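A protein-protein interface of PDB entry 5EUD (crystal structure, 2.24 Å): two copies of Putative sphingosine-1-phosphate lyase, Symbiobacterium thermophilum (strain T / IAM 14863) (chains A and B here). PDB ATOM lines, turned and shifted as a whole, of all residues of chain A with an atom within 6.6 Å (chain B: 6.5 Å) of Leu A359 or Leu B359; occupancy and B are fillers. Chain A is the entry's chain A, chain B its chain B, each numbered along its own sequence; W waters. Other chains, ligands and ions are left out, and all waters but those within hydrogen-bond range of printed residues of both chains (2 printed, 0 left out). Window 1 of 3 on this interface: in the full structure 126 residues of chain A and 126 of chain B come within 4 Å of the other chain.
The side-chain hydroxyl (OG1) of Thr B362 sits at hydrogen-bond distance from the backbone carbonyl oxygen (O) of Leu B359 (2.7 Å). N of Ala A317 sits at hydrogen-bond distance from OG1 of Thr A362, 3.1 Å away. OG1 of Thr B362 sits at hydrogen-bond distance from N of Ala B317 (3.2 Å). The backbone carbonyl oxygen (O) of Leu A359 is in hydrogen-bond range of the side-chain hydroxyl (OG1) of Thr A362 (2.7 Å).
Among the printed residues, pairs that only touch across the chains: Tyr A120 with Ala B317 (3.3 Å), Ala A317 with Tyr B120 (3.4 Å), Pro A356 with Lys B318 (3.4 Å), Lys A318 with Pro B356 (3.4 Å), Leu A359 with Tyr B120 (3.5 Å), Tyr A120 with Tyr B120 (3.5 Å), Tyr A120 with Leu B359 (3.6 Å), Pro A356 with Leu B359 (3.6 Å), Leu A359 with Pro B356 (3.7 Å) and Leu A359 with Leu B359 (3.95 Å).
Leu A359 touches just these residues of chain B: Tyr B120, Pro B356 and Leu B359. Leu B359 touches just these residues of chain A: Tyr A120 (3.6 Å), Pro A356 (3.6 Å) and Leu A359 (3.95 Å). Printed residues of chain B within 4 Å of Tyr A120: Tyr B120 (3.5 Å), Ala B317 (3.3 Å) and Leu B359 (3.6 Å). Printed residues of chain A within 4 Å of Tyr B120: Tyr A120, Ala A317 and Leu A359. Of the printed residues of chain B, Lys A318 touches Pro B356 (3.4 Å). Of the printed residues of chain A, Pro B356 touches Lys A318 (3.4 Å) and Leu A359 (3.7 Å). The nearest residue of chain B that does not touch Leu A359 is Lys B318 (6.3 Å). The nearest residue of chain A that does not touch Leu B359 is Lys A318 (6.3 Å). The nearest printed residue of chain A that does not touch Tyr B120 is Thr A362 (4.8 Å).
Of the 16 printed residues of chain B, 5 touch a printed residue of chain A. Hydrophobic or aromatic side chains of chain B that line the printed part of chain A: Tyr B120, Ala B317, Pro B356 and Leu B359. Hydrophobic or aromatic side chains of chain A within 4 Å of the printed part of chain B: Tyr A120, Ala A317, Pro A356 and Leu A359. Among the printed residues, no Asp or Glu carboxylate lies within 4 Å of a Lys or Arg side-chain nitrogen of the other chain.
Tyr B120 touches its own counterpart, Tyr A120. Lys A318 touches Pro B356, and with the chains exchanged Pro A356 touches Lys B318. Pro A356 touches Leu B359, and with the chains exchanged Leu A359 touches Pro B356. Leu A359 touches its own counterpart, Leu B359.
Water W1 bridges the side-chain hydroxyl of Tyr A120 (2.7 Å) and the backbone carbonyl oxygen of Lys B318 (3.0 Å). Water W2 lies within hydrogen-bond range of the side-chain hydroxyl of Tyr B120 and the backbone carbonyl oxygen of Lys A318.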
ATOM      1  N   TYR A 120      -6.691  24.407 -12.083  1.00  0.00           N
ATOM      2  CA  TYR A 120      -7.880  23.728 -11.600  1.00  0.00           C
ATOM      3  C   TYR A 120      -7.696  22.215 -11.748  1.00  0.00           C
ATOM      4  O   TYR A 120      -7.927  21.491 -10.795  1.00  0.00           O
ATOM      5  CB  TYR A 120      -9.140  24.174 -12.365  1.00  0.00           C
ATOM      6  CG  TYR A 120     -10.352  23.401 -11.889  1.00  0.00           C
ATOM      7  CD1 TYR A 120     -11.059  23.808 -10.760  1.00  0.00           C
ATOM      8  CD2 TYR A 120     -10.708  22.185 -12.479  1.00  0.00           C
ATOM      9  CE1 TYR A 120     -12.099  23.036 -10.237  1.00  0.00           C
ATOM     10  CE2 TYR A 120     -11.748  21.409 -11.968  1.00  0.00           C
ATOM     11  CZ  TYR A 120     -12.441  21.842 -10.845  1.00  0.00           C
ATOM     12  OH  TYR A 120     -13.487  21.114 -10.344  1.00  0.00           O
ATOM     13  N   GLN A 123      -5.397  20.514  -9.288  1.00  0.00           N
ATOM     14  CA  GLN A 123      -5.918  20.622  -7.931  1.00  0.00           C
ATOM     15  C   GLN A 123      -7.418  20.270  -7.785  1.00  0.00           C
ATOM     16  O   GLN A 123      -7.977  20.505  -6.711  1.00  0.00           O
ATOM     17  CB  GLN A 123      -5.668  22.057  -7.445  1.00  0.00           C
ATOM     18  CG  GLN A 123      -4.268  22.282  -6.887  1.00  0.00           C
ATOM     19  CD  GLN A 123      -4.243  22.102  -5.388  1.00  0.00           C
ATOM     20  OE1 GLN A 123      -4.991  22.761  -4.647  1.00  0.00           O
ATOM     21  NE2 GLN A 123      -3.359  21.235  -4.901  1.00  0.00           N
ATOM     22  N   VAL A 165      -9.742  32.839   3.162  1.00  0.00           N
ATOM     23  CA  VAL A 165     -10.225  32.841   1.788  1.00  0.00           C
ATOM     24  C   VAL A 165     -11.722  32.401   1.868  1.00  0.00           C
ATOM     25  O   VAL A 165     -12.037  31.447   2.574  1.00  0.00           O
ATOM     26  CB  VAL A 165      -9.360  31.912   0.865  1.00  0.00           C
ATOM     27  CG1 VAL A 165      -9.949  31.806  -0.541  1.00  0.00           C
ATOM     28  CG2 VAL A 165      -7.911  32.404   0.795  1.00  0.00           C
ATOM     29  N   THR A 310     -10.414  38.300  -4.875  1.00  0.00           N
ATOM     30  CA  THR A 310      -9.471  37.630  -5.761  1.00  0.00           C
ATOM     31  C   THR A 310     -10.185  37.254  -7.082  1.00  0.00           C
ATOM     32  O   THR A 310      -9.562  37.369  -8.128  1.00  0.00           O
ATOM     33  CB  THR A 310      -8.810  36.418  -5.089  1.00  0.00           C
ATOM     34  OG1 THR A 310      -9.776  35.681  -4.352  1.00  0.00           O
ATOM     35  CG2 THR A 310      -7.674  36.816  -4.171  1.00  0.00           C
ATOM     36  N   GLY A 316      -8.338  35.808 -10.400  1.00  0.00           N
ATOM     37  CA  GLY A 316      -8.467  34.390 -10.111  1.00  0.00           C
ATOM     38  C   GLY A 316      -9.750  33.881 -10.753  1.00  0.00           C
ATOM     39  O   GLY A 316     -10.525  34.670 -11.316  1.00  0.00           O
ATOM     40  N   ALA A 317      -9.996  32.574 -10.673  1.00  0.00           N
ATOM     41  CA  ALA A 317     -11.228  31.988 -11.214  1.00  0.00           C
ATOM     42  C   ALA A 317     -12.371  32.256 -10.260  1.00  0.00           C
ATOM     43  O   ALA A 317     -12.141  32.428  -9.074  1.00  0.00           O
ATOM     44  CB  ALA A 317     -11.070  30.484 -11.457  1.00  0.00           C
ATOM     45  N   LYS A 318     -13.603  32.286 -10.779  1.00  0.00           N
ATOM     46  CA  LYS A 318     -14.797  32.528  -9.987  1.00  0.00           C
ATOM     47  C   LYS A 318     -14.860  31.568  -8.801  1.00  0.00           C
ATOM     48  O   LYS A 318     -14.523  30.381  -8.943  1.00  0.00           O
ATOM     49  CB  LYS A 318     -16.074  32.409 -10.861  1.00  0.00           C
ATOM     50  CG  LYS A 318     -16.331  33.621 -11.756  1.00  0.00           C
ATOM     51  CD  LYS A 318     -16.656  34.895 -10.965  1.00  0.00           C
ATOM     52  CE  LYS A 318     -15.722  35.981 -11.414  1.00  0.00           C
ATOM     53  NZ  LYS A 318     -15.965  37.261 -10.694  1.00  0.00           N
ATOM     54  N   GLY A 319     -15.280  32.096  -7.652  1.00  0.00           N
ATOM     55  CA  GLY A 319     -15.425  31.287  -6.452  1.00  0.00           C
ATOM     56  C   GLY A 319     -14.474  31.624  -5.327  1.00  0.00           C
ATOM     57  O   GLY A 319     -14.399  30.857  -4.365  1.00  0.00           O
ATOM     58  N   THR A 320     -13.752  32.778  -5.396  1.00  0.00           N
ATOM     59  CA  THR A 320     -12.888  33.147  -4.260  1.00  0.00           C
ATOM     60  C   THR A 320     -12.935  34.637  -3.872  1.00  0.00           C
ATOM     61  O   THR A 320     -13.148  35.501  -4.711  1.00  0.00           O
ATOM     62  CB  THR A 320     -11.428  32.724  -4.448  1.00  0.00           C
ATOM     63  OG1 THR A 320     -10.876  33.494  -5.513  1.00  0.00           O
ATOM     64  CG2 THR A 320     -11.234  31.220  -4.646  1.00  0.00           C
ATOM     65  N   PRO A 356     -14.441  23.855  -2.725  1.00  0.00           N
ATOM     66  CA  PRO A 356     -13.655  23.526  -3.932  1.00  0.00           C
ATOM     67  C   PRO A 356     -12.245  24.139  -3.831  1.00  0.00           C
ATOM     68  O   PRO A 356     -12.030  25.283  -4.220  1.00  0.00           O
ATOM     69  CB  PRO A 356     -14.486  24.117  -5.076  1.00  0.00           C
ATOM     70  CG  PRO A 356     -15.289  25.210  -4.458  1.00  0.00           C
ATOM     71  CD  PRO A 356     -15.366  24.984  -2.967  1.00  0.00           C
ATOM     72  N   GLY A 357     -11.306  23.361  -3.285  1.00  0.00           N
ATOM     73  CA  GLY A 357      -9.925  23.779  -3.048  1.00  0.00           C
ATOM     74  C   GLY A 357      -9.172  24.242  -4.265  1.00  0.00           C
ATOM     75  O   GLY A 357      -8.313  25.111  -4.159  1.00  0.00           O
ATOM     76  N   ALA A 358      -9.506  23.680  -5.432  1.00  0.00           N
ATOM     77  CA  ALA A 358      -8.902  24.031  -6.712  1.00  0.00           C
ATOM     78  C   ALA A 358      -9.051  25.516  -7.051  1.00  0.00           C
ATOM     79  O   ALA A 358      -8.209  26.038  -7.779  1.00  0.00           O
ATOM     80  CB  ALA A 358      -9.534  23.198  -7.810  1.00  0.00           C
ATOM     81  N   LEU A 359     -10.134  26.182  -6.574  1.00  0.00           N
ATOM     82  CA  LEU A 359     -10.384  27.600  -6.861  1.00  0.00           C
ATOM     83  C   LEU A 359      -9.469  28.510  -6.087  1.00  0.00           C
ATOM     84  O   LEU A 359      -9.119  29.567  -6.599  1.00  0.00           O
ATOM     85  CB  LEU A 359     -11.857  27.993  -6.685  1.00  0.00           C
ATOM     86  CG  LEU A 359     -12.874  27.160  -7.504  1.00  0.00           C
ATOM     87  CD1 LEU A 359     -14.277  27.551  -7.158  1.00  0.00           C
ATOM     88  CD2 LEU A 359     -12.622  27.297  -9.021  1.00  0.00           C
ATOM     89  N   SER A 360      -9.049  28.085  -4.874  1.00  0.00           N
ATOM     90  CA  SER A 360      -8.083  28.793  -4.030  1.00  0.00           C
ATOM     91  C   SER A 360      -6.724  28.779  -4.707  1.00  0.00           C
ATOM     92  O   SER A 360      -6.008  29.789  -4.676  1.00  0.00           O
ATOM     93  CB  SER A 360      -7.981  28.115  -2.672  1.00  0.00           C
ATOM     94  OG  SER A 360      -9.194  28.318  -1.967  1.00  0.00           O
ATOM     95  N   ALA A 361      -6.373  27.613  -5.322  1.00  0.00           N
ATOM     96  CA  ALA A 361      -5.171  27.410  -6.104  1.00  0.00           C
ATOM     97  C   ALA A 361      -5.164  28.370  -7.307  1.00  0.00           C
ATOM     98  O   ALA A 361      -4.136  28.990  -7.539  1.00  0.00           O
ATOM     99  CB  ALA A 361      -5.077  25.961  -6.572  1.00  0.00           C
ATOM    100  N   THR A 362      -6.312  28.573  -8.010  1.00  0.00           N
ATOM    101  CA  THR A 362      -6.379  29.514  -9.168  1.00  0.00           C
ATOM    102  C   THR A 362      -6.105  30.950  -8.722  1.00  0.00           C
ATOM    103  O   THR A 362      -5.449  31.697  -9.455  1.00  0.00           O
ATOM    104  CB  THR A 362      -7.701  29.461  -9.964  1.00  0.00           C
ATOM    105  OG1 THR A 362      -8.745  30.080  -9.220  1.00  0.00           O
ATOM    106  CG2 THR A 362      -8.102  28.054 -10.399  1.00  0.00           C
ATOM    107  N   ALA A 363      -6.573  31.315  -7.508  1.00  0.00           N
ATOM    108  CA  ALA A 363      -6.356  32.652  -6.932  1.00  0.00           C
ATOM    109  C   ALA A 363      -4.862  32.869  -6.644  1.00  0.00           C
ATOM    110  O   ALA A 363      -4.330  33.919  -7.001  1.00  0.00           O
ATOM    111  CB  ALA A 363      -7.181  32.843  -5.660  1.00  0.00           C
ATOM    112  N   TRP A 364      -4.188  31.863  -6.022  1.00  0.00           N
ATOM    113  CA  TRP A 364      -2.763  31.876  -5.694  1.00  0.00           C
ATOM    114  C   TRP A 364      -1.951  31.938  -6.992  1.00  0.00           C
ATOM    115  O   TRP A 364      -1.070  32.786  -7.114  1.00  0.00           O
ATOM    116  CB  TRP A 364      -2.448  30.606  -4.901  1.00  0.00           C
ATOM    117  CG  TRP A 364      -1.031  30.435  -4.451  1.00  0.00           C
ATOM    118  CD1 TRP A 364      -0.469  30.936  -3.313  1.00  0.00           C
ATOM    119  CD2 TRP A 364      -0.044  29.565  -5.040  1.00  0.00           C
ATOM    120  NE1 TRP A 364       0.821  30.480  -3.184  1.00  0.00           N
ATOM    121  CE2 TRP A 364       1.099  29.613  -4.215  1.00  0.00           C
ATOM    122  CE3 TRP A 364      -0.028  28.723  -6.167  1.00  0.00           C
ATOM    123  CZ2 TRP A 364       2.259  28.871  -4.494  1.00  0.00           C
ATOM    124  CZ3 TRP A 364       1.136  28.020  -6.461  1.00  0.00           C
ATOM    125  CH2 TRP A 364       2.255  28.088  -5.622  1.00  0.00           C
ATOM    126  N   TYR B 120     -15.122  21.687 -16.747  1.00  0.00           N
ATOM    127  CA  TYR B 120     -14.716  22.894 -16.019  1.00  0.00           C
ATOM    128  C   TYR B 120     -14.126  23.899 -17.017  1.00  0.00           C
ATOM    129  O   TYR B 120     -14.609  25.014 -17.079  1.00  0.00           O
ATOM    130  CB  TYR B 120     -13.686  22.594 -14.894  1.00  0.00           C
ATOM    131  CG  TYR B 120     -13.268  23.868 -14.202  1.00  0.00           C
ATOM    132  CD1 TYR B 120     -13.971  24.344 -13.095  1.00  0.00           C
ATOM    133  CD2 TYR B 120     -12.256  24.679 -14.734  1.00  0.00           C
ATOM    134  CE1 TYR B 120     -13.700  25.601 -12.551  1.00  0.00           C
ATOM    135  CE2 TYR B 120     -11.944  25.916 -14.164  1.00  0.00           C
ATOM    136  CZ  TYR B 120     -12.674  26.373 -13.076  1.00  0.00           C
ATOM    137  OH  TYR B 120     -12.398  27.588 -12.515  1.00  0.00           O
ATOM    138  N   GLN B 123     -16.594  25.781 -19.204  1.00  0.00           N
ATOM    139  CA  GLN B 123     -17.494  26.662 -18.461  1.00  0.00           C
ATOM    140  C   GLN B 123     -16.764  27.524 -17.412  1.00  0.00           C
ATOM    141  O   GLN B 123     -17.429  28.167 -16.585  1.00  0.00           O
ATOM    142  CB  GLN B 123     -18.530  25.772 -17.746  1.00  0.00           C
ATOM    143  CG  GLN B 123     -19.635  25.270 -18.658  1.00  0.00           C
ATOM    144  CD  GLN B 123     -20.851  26.149 -18.544  1.00  0.00           C
ATOM    145  OE1 GLN B 123     -21.502  26.239 -17.484  1.00  0.00           O
ATOM    146  NE2 GLN B 123     -21.152  26.855 -19.621  1.00  0.00           N
ATOM    147  N   GLY B 316     -19.966  14.537  -8.930  1.00  0.00           N
ATOM    148  CA  GLY B 316     -19.659  15.847  -9.502  1.00  0.00           C
ATOM    149  C   GLY B 316     -18.405  16.385  -8.831  1.00  0.00           C
ATOM    150  O   GLY B 316     -17.952  15.814  -7.829  1.00  0.00           O
ATOM    151  N   ALA B 317     -17.817  17.459  -9.350  1.00  0.00           N
ATOM    152  CA  ALA B 317     -16.619  17.997  -8.690  1.00  0.00           C
ATOM    153  C   ALA B 317     -17.001  18.740  -7.383  1.00  0.00           C
ATOM    154  O   ALA B 317     -18.146  19.157  -7.242  1.00  0.00           O
ATOM    155  CB  ALA B 317     -15.870  18.922  -9.630  1.00  0.00           C
ATOM    156  N   LYS B 318     -16.054  18.887  -6.429  1.00  0.00           N
ATOM    157  CA  LYS B 318     -16.282  19.601  -5.166  1.00  0.00           C
ATOM    158  C   LYS B 318     -16.873  21.005  -5.415  1.00  0.00           C
ATOM    159  O   LYS B 318     -16.468  21.690  -6.353  1.00  0.00           O
ATOM    160  CB  LYS B 318     -14.968  19.741  -4.368  1.00  0.00           C
ATOM    161  CG  LYS B 318     -14.412  18.440  -3.811  1.00  0.00           C
ATOM    162  CD  LYS B 318     -15.204  17.978  -2.618  1.00  0.00           C
ATOM    163  CE  LYS B 318     -15.885  16.679  -2.893  1.00  0.00           C
ATOM    164  NZ  LYS B 318     -16.781  16.311  -1.768  1.00  0.00           N
ATOM    165  N   GLY B 319     -17.826  21.401  -4.591  1.00  0.00           N
ATOM    166  CA  GLY B 319     -18.428  22.720  -4.695  1.00  0.00           C
ATOM    167  C   GLY B 319     -19.903  22.770  -5.025  1.00  0.00           C
ATOM    168  O   GLY B 319     -20.400  23.850  -5.347  1.00  0.00           O
ATOM    169  N   THR B 320     -20.621  21.626  -4.977  1.00  0.00           N
ATOM    170  CA  THR B 320     -22.066  21.615  -5.277  1.00  0.00           C
ATOM    171  C   THR B 320     -22.846  20.639  -4.397  1.00  0.00           C
ATOM    172  O   THR B 320     -22.360  19.566  -4.028  1.00  0.00           O
ATOM    173  CB  THR B 320     -22.391  21.288  -6.765  1.00  0.00           C
ATOM    174  OG1 THR B 320     -21.933  19.975  -7.074  1.00  0.00           O
ATOM    175  CG2 THR B 320     -21.876  22.318  -7.772  1.00  0.00           C
ATOM    176  N   PRO B 356     -19.156  29.895  -8.766  1.00  0.00           N
ATOM    177  CA  PRO B 356     -18.395  29.210  -9.819  1.00  0.00           C
ATOM    178  C   PRO B 356     -19.306  28.295 -10.651  1.00  0.00           C
ATOM    179  O   PRO B 356     -19.396  27.093 -10.378  1.00  0.00           O
ATOM    180  CB  PRO B 356     -17.342  28.441  -9.020  1.00  0.00           C
ATOM    181  CG  PRO B 356     -18.007  28.154  -7.688  1.00  0.00           C
ATOM    182  CD  PRO B 356     -19.064  29.180  -7.466  1.00  0.00           C
ATOM    183  N   GLY B 357     -19.962  28.865 -11.671  1.00  0.00           N
ATOM    184  CA  GLY B 357     -20.872  28.137 -12.556  1.00  0.00           C
ATOM    185  C   GLY B 357     -20.330  26.872 -13.179  1.00  0.00           C
ATOM    186  O   GLY B 357     -21.086  25.953 -13.467  1.00  0.00           O
ATOM    187  N   ALA B 358     -19.012  26.801 -13.372  1.00  0.00           N
ATOM    188  CA  ALA B 358     -18.349  25.617 -13.920  1.00  0.00           C
ATOM    189  C   ALA B 358     -18.563  24.380 -13.043  1.00  0.00           C
ATOM    190  O   ALA B 358     -18.588  23.285 -13.580  1.00  0.00           O
ATOM    191  CB  ALA B 358     -16.870  25.883 -14.077  1.00  0.00           C
ATOM    192  N   LEU B 359     -18.689  24.541 -11.701  1.00  0.00           N
ATOM    193  CA  LEU B 359     -18.909  23.402 -10.799  1.00  0.00           C
ATOM    194  C   LEU B 359     -20.298  22.783 -10.979  1.00  0.00           C
ATOM    195  O   LEU B 359     -20.415  21.566 -10.928  1.00  0.00           O
ATOM    196  CB  LEU B 359     -18.599  23.749  -9.336  1.00  0.00           C
ATOM    197  CG  LEU B 359     -17.192  24.354  -9.110  1.00  0.00           C
ATOM    198  CD1 LEU B 359     -16.983  24.717  -7.664  1.00  0.00           C
ATOM    199  CD2 LEU B 359     -16.074  23.447  -9.642  1.00  0.00           C
ATOM    200  N   SER B 360     -21.323  23.607 -11.282  1.00  0.00           N
ATOM    201  CA  SER B 360     -22.678  23.159 -11.618  1.00  0.00           C
ATOM    202  C   SER B 360     -22.633  22.351 -12.924  1.00  0.00           C
ATOM    203  O   SER B 360     -23.376  21.374 -13.072  1.00  0.00           O
ATOM    204  CB  SER B 360     -23.582  24.361 -11.852  1.00  0.00           C
ATOM    205  OG  SER B 360     -23.756  25.030 -10.619  1.00  0.00           O
ATOM    206  N   ALA B 361     -21.789  22.787 -13.877  1.00  0.00           N
ATOM    207  CA  ALA B 361     -21.631  22.088 -15.147  1.00  0.00           C
ATOM    208  C   ALA B 361     -21.004  20.711 -14.893  1.00  0.00           C
ATOM    209  O   ALA B 361     -21.418  19.752 -15.528  1.00  0.00           O
ATOM    210  CB  ALA B 361     -20.769  22.892 -16.102  1.00  0.00           C
ATOM    211  N   THR B 362     -20.040  20.600 -13.951  1.00  0.00           N
ATOM    212  CA  THR B 362     -19.438  19.291 -13.666  1.00  0.00           C
ATOM    213  C   THR B 362     -20.470  18.348 -13.037  1.00  0.00           C
ATOM    214  O   THR B 362     -20.400  17.146 -13.278  1.00  0.00           O
ATOM    215  CB  THR B 362     -18.189  19.390 -12.791  1.00  0.00           C
ATOM    216  OG1 THR B 362     -18.596  19.691 -11.440  1.00  0.00           O
ATOM    217  CG2 THR B 362     -17.125  20.402 -13.347  1.00  0.00           C
ATOM    218  N   ALA B 363     -21.422  18.891 -12.236  1.00  0.00           N
ATOM    219  CA  ALA B 363     -22.487  18.099 -11.586  1.00  0.00           C
ATOM    220  C   ALA B 363     -23.447  17.584 -12.671  1.00  0.00           C
ATOM    221  O   ALA B 363     -23.804  16.417 -12.649  1.00  0.00           O
ATOM    222  CB  ALA B 363     -23.249  18.951 -10.582  1.00  0.00           C
ATOM    223  N   TRP B 364     -23.816  18.457 -13.643  1.00  0.00           N
ATOM    224  CA  TRP B 364     -24.708  18.136 -14.747  1.00  0.00           C
ATOM    225  C   TRP B 364     -24.090  17.053 -15.627  1.00  0.00           C
ATOM    226  O   TRP B 364     -24.748  16.038 -15.901  1.00  0.00           O
ATOM    227  CB  TRP B 364     -25.029  19.405 -15.547  1.00  0.00           C
ATOM    228  CG  TRP B 364     -25.962  19.208 -16.708  1.00  0.00           C
ATOM    229  CD1 TRP B 364     -27.326  19.289 -16.686  1.00  0.00           C
ATOM    230  CD2 TRP B 364     -25.585  19.172 -18.100  1.00  0.00           C
ATOM    231  NE1 TRP B 364     -27.823  19.224 -17.971  1.00  0.00           N
ATOM    232  CE2 TRP B 364     -26.777  19.154 -18.856  1.00  0.00           C
ATOM    233  CE3 TRP B 364     -24.349  19.161 -18.776  1.00  0.00           C
ATOM    234  CZ2 TRP B 364     -26.774  19.092 -20.261  1.00  0.00           C
ATOM    235  CZ3 TRP B 364     -24.347  19.088 -20.165  1.00  0.00           C
ATOM    236  CH2 TRP B 364     -25.547  19.036 -20.892  1.00  0.00           C
HETATM  237  O   HOH W   1     -13.803  21.735  -7.718  1.00  0.00           O
HETATM  238  O   HOH W   2     -14.533  29.010 -11.494  1.00  0.00           O
